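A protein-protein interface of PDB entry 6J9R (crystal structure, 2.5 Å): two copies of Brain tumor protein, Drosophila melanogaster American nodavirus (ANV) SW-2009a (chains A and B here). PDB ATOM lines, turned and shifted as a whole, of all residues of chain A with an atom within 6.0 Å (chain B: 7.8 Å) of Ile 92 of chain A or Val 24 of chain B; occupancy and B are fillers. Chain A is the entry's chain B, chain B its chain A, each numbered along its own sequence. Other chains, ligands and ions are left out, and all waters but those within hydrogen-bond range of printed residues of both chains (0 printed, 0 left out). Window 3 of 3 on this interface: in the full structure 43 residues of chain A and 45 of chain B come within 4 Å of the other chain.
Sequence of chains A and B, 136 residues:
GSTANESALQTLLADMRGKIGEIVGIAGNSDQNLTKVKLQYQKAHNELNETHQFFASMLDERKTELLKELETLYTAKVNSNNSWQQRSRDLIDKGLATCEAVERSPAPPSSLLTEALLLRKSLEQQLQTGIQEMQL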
ATOM      1  N   ARG A  87      -8.334  -7.275  -1.488  1.00  0.00           N
ATOM      2  CA  ARG A  87      -7.473  -8.291  -2.079  1.00  0.00           C
ATOM      3  C   ARG A  87      -7.864  -9.666  -1.539  1.00  0.00           C
ATOM      4  O   ARG A  87      -7.883 -10.642  -2.284  1.00  0.00           O
ATOM      5  CB  ARG A  87      -6.004  -7.980  -1.789  1.00  0.00           C
ATOM      6  CG  ARG A  87      -5.023  -9.120  -2.050  1.00  0.00           C
ATOM      7  CD  ARG A  87      -3.625  -8.625  -2.416  1.00  0.00           C
ATOM      8  NE  ARG A  87      -2.661  -9.722  -2.529  1.00  0.00           N
ATOM      9  CZ  ARG A  87      -2.445 -10.470  -3.613  1.00  0.00           C
ATOM     10  NH1 ARG A  87      -3.111 -10.255  -4.745  1.00  0.00           N
ATOM     11  NH2 ARG A  87      -1.541 -11.443  -3.559  1.00  0.00           N
ATOM     12  N   SER A  88      -8.205  -9.731  -0.252  1.00  0.00           N
ATOM     13  CA  SER A  88      -8.684 -10.976   0.338  1.00  0.00           C
ATOM     14  C   SER A  88     -10.005 -11.455  -0.300  1.00  0.00           C
ATOM     15  O   SER A  88     -10.143 -12.638  -0.611  1.00  0.00           O
ATOM     16  CB  SER A  88      -8.863 -10.819   1.849  1.00  0.00           C
ATOM     17  OG  SER A  88      -7.613 -10.866   2.522  1.00  0.00           O
ATOM     18  N   ARG A  89     -10.958 -10.551  -0.522  1.00  0.00           N
ATOM     19  CA  ARG A  89     -12.207 -10.947  -1.173  1.00  0.00           C
ATOM     20  C   ARG A  89     -11.931 -11.530  -2.559  1.00  0.00           C
ATOM     21  O   ARG A  89     -12.549 -12.507  -2.971  1.00  0.00           O
ATOM     22  CB  ARG A  89     -13.171  -9.771  -1.300  1.00  0.00           C
ATOM     23  CG  ARG A  89     -13.578  -9.154   0.019  1.00  0.00           C
ATOM     24  CD  ARG A  89     -14.815  -8.287  -0.152  1.00  0.00           C
ATOM     25  NE  ARG A  89     -15.328  -7.779   1.124  1.00  0.00           N
ATOM     26  N   ASP A  90     -10.986 -10.935  -3.267  1.00  0.00           N
ATOM     27  CA  ASP A  90     -10.665 -11.389  -4.609  1.00  0.00           C
ATOM     28  C   ASP A  90      -9.859 -12.690  -4.614  1.00  0.00           C
ATOM     29  O   ASP A  90     -10.028 -13.497  -5.505  1.00  0.00           O
ATOM     30  CB  ASP A  90      -9.980 -10.250  -5.376  1.00  0.00           C
ATOM     31  CG  ASP A  90     -10.993  -9.140  -5.754  1.00  0.00           C
ATOM     32  OD1 ASP A  90     -12.101  -9.481  -6.246  1.00  0.00           O
ATOM     33  OD2 ASP A  90     -10.725  -7.943  -5.510  1.00  0.00           O
ATOM     34  N   LEU A  91      -8.995 -12.895  -3.623  1.00  0.00           N
ATOM     35  CA  LEU A  91      -8.251 -14.150  -3.500  1.00  0.00           C
ATOM     36  C   LEU A  91      -9.147 -15.307  -3.074  1.00  0.00           C
ATOM     37  O   LEU A  91      -9.002 -16.437  -3.548  1.00  0.00           O
ATOM     38  CB  LEU A  91      -7.105 -14.005  -2.502  1.00  0.00           C
ATOM     39  CG  LEU A  91      -5.831 -13.325  -3.001  1.00  0.00           C
ATOM     40  CD1 LEU A  91      -4.767 -13.214  -1.876  1.00  0.00           C
ATOM     41  CD2 LEU A  91      -5.287 -14.088  -4.205  1.00  0.00           C
ATOM     42  N   ILE A  92     -10.056 -15.031  -2.150  1.00  0.00           N
ATOM     43  CA  ILE A  92     -11.006 -16.043  -1.713  1.00  0.00           C
ATOM     44  C   ILE A  92     -11.858 -16.473  -2.890  1.00  0.00           C
ATOM     45  O   ILE A  92     -12.026 -17.652  -3.130  1.00  0.00           O
ATOM     46  CB  ILE A  92     -11.907 -15.511  -0.602  1.00  0.00           C
ATOM     47  CG1 ILE A  92     -11.107 -15.299   0.689  1.00  0.00           C
ATOM     48  CG2 ILE A  92     -13.086 -16.429  -0.377  1.00  0.00           C
ATOM     49  CD1 ILE A  92     -11.814 -14.376   1.666  1.00  0.00           C
ATOM     50  N   ASP A  93     -12.325 -15.494  -3.668  1.00  0.00           N
ATOM     51  CA  ASP A  93     -13.153 -15.757  -4.828  1.00  0.00           C
ATOM     52  C   ASP A  93     -12.412 -16.595  -5.851  1.00  0.00           C
ATOM     53  O   ASP A  93     -12.943 -17.593  -6.348  1.00  0.00           O
ATOM     54  CB  ASP A  93     -13.602 -14.433  -5.465  1.00  0.00           C
ATOM     55  CG  ASP A  93     -14.432 -14.640  -6.710  1.00  0.00           C
ATOM     56  OD1 ASP A  93     -15.627 -14.988  -6.570  1.00  0.00           O
ATOM     57  OD2 ASP A  93     -13.891 -14.465  -7.827  1.00  0.00           O
ATOM     58  N   LYS A  94     -11.174 -16.200  -6.126  1.00  0.00           N
ATOM     59  CA  LYS A  94     -10.353 -16.851  -7.129  1.00  0.00           C
ATOM     60  C   LYS A  94      -9.872 -18.209  -6.599  1.00  0.00           C
ATOM     61  O   LYS A  94      -9.877 -19.227  -7.317  1.00  0.00           O
ATOM     62  CB  LYS A  94      -9.175 -15.935  -7.502  1.00  0.00           C
ATOM     63  CG  LYS A  94      -8.678 -16.064  -8.929  1.00  0.00           C
ATOM     64  N   GLY A  95      -9.502 -18.228  -5.318  1.00  0.00           N
ATOM     65  CA  GLY A  95      -9.003 -19.434  -4.679  1.00  0.00           C
ATOM     66  C   GLY A  95     -10.056 -20.507  -4.704  1.00  0.00           C
ATOM     67  O   GLY A  95      -9.791 -21.621  -5.131  1.00  0.00           O
ATOM     68  N   LEU A  96     -11.276 -20.155  -4.324  1.00  0.00           N
ATOM     69  CA  LEU A  96     -12.388 -21.114  -4.356  1.00  0.00           C
ATOM     70  C   LEU A  96     -12.668 -21.660  -5.737  1.00  0.00           C
ATOM     71  O   LEU A  96     -12.734 -22.869  -5.914  1.00  0.00           O
ATOM     72  CB  LEU A  96     -13.664 -20.461  -3.841  1.00  0.00           C
ATOM     73  CG  LEU A  96     -14.056 -20.674  -2.377  1.00  0.00           C
ATOM     74  CD1 LEU A  96     -12.970 -21.379  -1.589  1.00  0.00           C
ATOM     75  CD2 LEU A  96     -14.432 -19.371  -1.741  1.00  0.00           C
ATOM     76  N   ALA A  97     -12.776 -20.775  -6.722  1.00  0.00           N
ATOM     77  CA  ALA A  97     -13.080 -21.203  -8.082  1.00  0.00           C
ATOM     78  C   ALA A  97     -12.012 -22.169  -8.610  1.00  0.00           C
ATOM     79  O   ALA A  97     -12.330 -23.166  -9.259  1.00  0.00           O
ATOM     80  CB  ALA A  97     -13.207 -19.994  -9.000  1.00  0.00           C
ATOM     81  N   LEU A 123      -2.307 -16.855  -1.107  1.00  0.00           N
ATOM     82  CA  LEU A 123      -3.087 -17.026   0.099  1.00  0.00           C
ATOM     83  C   LEU A 123      -2.196 -17.055   1.334  1.00  0.00           C
ATOM     84  O   LEU A 123      -2.545 -16.481   2.361  1.00  0.00           O
ATOM     85  CB  LEU A 123      -3.920 -18.313   0.052  1.00  0.00           C
ATOM     86  CG  LEU A 123      -5.180 -18.501  -0.811  1.00  0.00           C
ATOM     87  CD1 LEU A 123      -5.551 -17.266  -1.614  1.00  0.00           C
ATOM     88  CD2 LEU A 123      -5.120 -19.739  -1.684  1.00  0.00           C
ATOM     89  N   ARG B  17      -7.867 -24.561   0.772  1.00  0.00           N
ATOM     90  CA  ARG B  17      -9.160 -24.299   1.403  1.00  0.00           C
ATOM     91  C   ARG B  17      -8.974 -23.948   2.875  1.00  0.00           C
ATOM     92  O   ARG B  17      -9.715 -23.117   3.431  1.00  0.00           O
ATOM     93  CB  ARG B  17     -10.098 -25.492   1.234  1.00  0.00           C
ATOM     94  CG  ARG B  17     -10.517 -25.758  -0.215  1.00  0.00           C
ATOM     95  CD  ARG B  17     -11.615 -26.836  -0.246  1.00  0.00           C
ATOM     96  NE  ARG B  17     -12.100 -27.148  -1.588  1.00  0.00           N
ATOM     97  CZ  ARG B  17     -13.085 -26.486  -2.198  1.00  0.00           C
ATOM     98  NH1 ARG B  17     -13.492 -26.845  -3.413  1.00  0.00           N
ATOM     99  NH2 ARG B  17     -13.677 -25.470  -1.586  1.00  0.00           N
ATOM    100  N   GLY B  18      -7.952 -24.527   3.495  1.00  0.00           N
ATOM    101  CA  GLY B  18      -7.652 -24.188   4.870  1.00  0.00           C
ATOM    102  C   GLY B  18      -7.215 -22.738   4.995  1.00  0.00           C
ATOM    103  O   GLY B  18      -7.637 -22.010   5.897  1.00  0.00           O
ATOM    104  N   LYS B  19      -6.362 -22.297   4.088  1.00  0.00           N
ATOM    105  CA  LYS B  19      -5.884 -20.935   4.160  1.00  0.00           C
ATOM    106  C   LYS B  19      -7.012 -19.978   3.839  1.00  0.00           C
ATOM    107  O   LYS B  19      -7.132 -18.932   4.463  1.00  0.00           O
ATOM    108  CB  LYS B  19      -4.700 -20.732   3.218  1.00  0.00           C
ATOM    109  CG  LYS B  19      -3.395 -21.235   3.800  1.00  0.00           C
ATOM    110  CD  LYS B  19      -2.312 -21.348   2.744  1.00  0.00           C
ATOM    111  CE  LYS B  19      -0.981 -21.790   3.350  1.00  0.00           C
ATOM    112  NZ  LYS B  19      -1.159 -23.080   4.033  1.00  0.00           N
ATOM    113  N   ILE B  20      -7.867 -20.354   2.898  1.00  0.00           N
ATOM    114  CA  ILE B  20      -9.028 -19.530   2.571  1.00  0.00           C
ATOM    115  C   ILE B  20      -9.911 -19.334   3.805  1.00  0.00           C
ATOM    116  O   ILE B  20     -10.272 -18.208   4.143  1.00  0.00           O
ATOM    117  CB  ILE B  20      -9.835 -20.153   1.436  1.00  0.00           C
ATOM    118  CG1 ILE B  20      -9.117 -19.876   0.106  1.00  0.00           C
ATOM    119  CG2 ILE B  20     -11.229 -19.574   1.413  1.00  0.00           C
ATOM    120  CD1 ILE B  20      -9.657 -20.628  -1.082  1.00  0.00           C
ATOM    121  N   GLY B  21     -10.206 -20.421   4.509  1.00  0.00           N
ATOM    122  CA  GLY B  21     -10.992 -20.328   5.726  1.00  0.00           C
ATOM    123  C   GLY B  21     -10.347 -19.450   6.785  1.00  0.00           C
ATOM    124  O   GLY B  21     -11.036 -18.683   7.452  1.00  0.00           O
ATOM    125  N   GLU B  22      -9.035 -19.588   6.964  1.00  0.00           N
ATOM    126  CA  GLU B  22      -8.288 -18.747   7.907  1.00  0.00           C
ATOM    127  C   GLU B  22      -8.410 -17.254   7.568  1.00  0.00           C
ATOM    128  O   GLU B  22      -8.673 -16.420   8.442  1.00  0.00           O
ATOM    129  CB  GLU B  22      -6.802 -19.160   7.949  1.00  0.00           C
ATOM    130  CG  GLU B  22      -6.519 -20.513   8.634  1.00  0.00           C
ATOM    131  CD  GLU B  22      -5.043 -20.894   8.628  1.00  0.00           C
ATOM    132  OE1 GLU B  22      -4.265 -20.235   9.344  1.00  0.00           O
ATOM    133  OE2 GLU B  22      -4.658 -21.851   7.912  1.00  0.00           O
ATOM    134  N   ILE B  23      -8.194 -16.921   6.303  1.00  0.00           N
ATOM    135  CA  ILE B  23      -8.326 -15.539   5.838  1.00  0.00           C
ATOM    136  C   ILE B  23      -9.729 -15.001   6.100  1.00  0.00           C
ATOM    137  O   ILE B  23      -9.893 -13.886   6.571  1.00  0.00           O
ATOM    138  CB  ILE B  23      -7.989 -15.434   4.353  1.00  0.00           C
ATOM    139  CG1 ILE B  23      -6.479 -15.510   4.162  1.00  0.00           C
ATOM    140  CG2 ILE B  23      -8.553 -14.139   3.745  1.00  0.00           C
ATOM    141  CD1 ILE B  23      -6.075 -15.877   2.759  1.00  0.00           C
ATOM    142  N   VAL B  24     -10.734 -15.810   5.783  1.00  0.00           N
ATOM    143  CA  VAL B  24     -12.124 -15.456   6.001  1.00  0.00           C
ATOM    144  C   VAL B  24     -12.331 -15.124   7.472  1.00  0.00           C
ATOM    145  O   VAL B  24     -12.920 -14.096   7.814  1.00  0.00           O
ATOM    146  CB  VAL B  24     -13.056 -16.592   5.573  1.00  0.00           C
ATOM    147  CG1 VAL B  24     -14.433 -16.420   6.207  1.00  0.00           C
ATOM    148  CG2 VAL B  24     -13.128 -16.669   4.032  1.00  0.00           C
ATOM    149  N   GLY B  25     -11.785 -15.959   8.344  1.00  0.00           N
ATOM    150  CA  GLY B  25     -11.829 -15.674   9.765  1.00  0.00           C
ATOM    151  C   GLY B  25     -11.084 -14.411  10.155  1.00  0.00           C
ATOM    152  O   GLY B  25     -11.685 -13.483  10.700  1.00  0.00           O
ATOM    153  N   ILE B  26      -9.782 -14.364   9.864  1.00  0.00           N
ATOM    154  CA  ILE B  26      -8.943 -13.222  10.247  1.00  0.00           C
ATOM    155  C   ILE B  26      -9.297 -11.940   9.490  1.00  0.00           C
ATOM    156  O   ILE B  26      -8.650 -10.917   9.685  1.00  0.00           O
ATOM    157  CB  ILE B  26      -7.430 -13.509  10.028  1.00  0.00           C
ATOM    158  N   ALA B  27     -10.305 -11.985   8.624  1.00  0.00           N
ATOM    159  CA  ALA B  27     -10.769 -10.755   8.016  1.00  0.00           C
ATOM    160  C   ALA B  27     -11.653 -10.074   9.031  1.00  0.00           C
ATOM    161  O   ALA B  27     -11.764  -8.840   9.044  1.00  0.00           O
ATOM    162  CB  ALA B  27     -11.523 -11.001   6.695  1.00  0.00           C
ATOM    163  N   GLY B  28     -12.270 -10.869   9.905  1.00  0.00           N
ATOM    164  CA  GLY B  28     -13.035 -10.295  11.003  1.00  0.00           C
ATOM    165  C   GLY B  28     -14.218  -9.565  10.409  1.00  0.00           C
ATOM    166  O   GLY B  28     -14.553  -9.783   9.246  1.00  0.00           O
ATOM    167  N   ASN B  29     -14.910  -8.773  11.217  1.00  0.00           N
ATOM    168  CA  ASN B  29     -15.833  -7.790  10.674  1.00  0.00           C
ATOM    169  C   ASN B  29     -15.017  -6.593  10.178  1.00  0.00           C
ATOM    170  O   ASN B  29     -14.476  -5.845  10.988  1.00  0.00           O
ATOM    171  CB  ASN B  29     -16.845  -7.377  11.750  1.00  0.00           C
ATOM    172  CG  ASN B  29     -18.022  -6.593  11.194  1.00  0.00           C
ATOM    173  OD1 ASN B  29     -17.903  -5.872  10.200  1.00  0.00           O
ATOM    174  ND2 ASN B  29     -19.172  -6.730  11.845  1.00  0.00           N
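Ile 23 of chain B touches Ser 88 of chain A (CG2 to OG, 3.6 Å). Ile 23 of chain B touches Ile 92 of chain A. CG2 of Val 24 of chain B touches CD1 of Ile 92 of chain A (3.5 Å). Gly 95 of chain A touches Ile 20 of chain B (C to CD1, 3.6 Å). Leu 96 of chain A touches Ile 20 of chain B (CD1 to CD1, 3.4 Å). Leu 123 of chain A touches Ile 23 of chain B (O to CD1, 3.6 Å).
No position is printed for both chains. Of the 6 pairs that touch across the chains among the printed residues, none has its exchanged pair printed and touching as well.
Of the 13 printed residues of chain B, 3 touch a printed residue of chain A. Among the printed residues, no Asp or Glu carboxylate lies within 4 Å of a Lys or Arg side-chain nitrogen of the other chain.
Printed residues of chain B within 4 Å of Ile 92 of chain A: Ile 23 (3.9 Å) and Val 24 (3.5 Å). Lys 94 of chain A touches none of the printed residues of chain B. Of the printed residues of chain B, Gly 95 of chain A touches Ile 20. Of the printed residues of chain B, Leu 123 of chain A touches Ile 23 (3.6 Å). Arg 17 of chain B touches none of the printed residues of chain A. The nearest printed residue of chain A that does not touch Val 24 of chain B is Leu 96 of chain A (6.5 Å). The nearest printed residue of chain A that does not touch Ile 23 of chain B is Leu 91 of chain A (5.5 Å).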
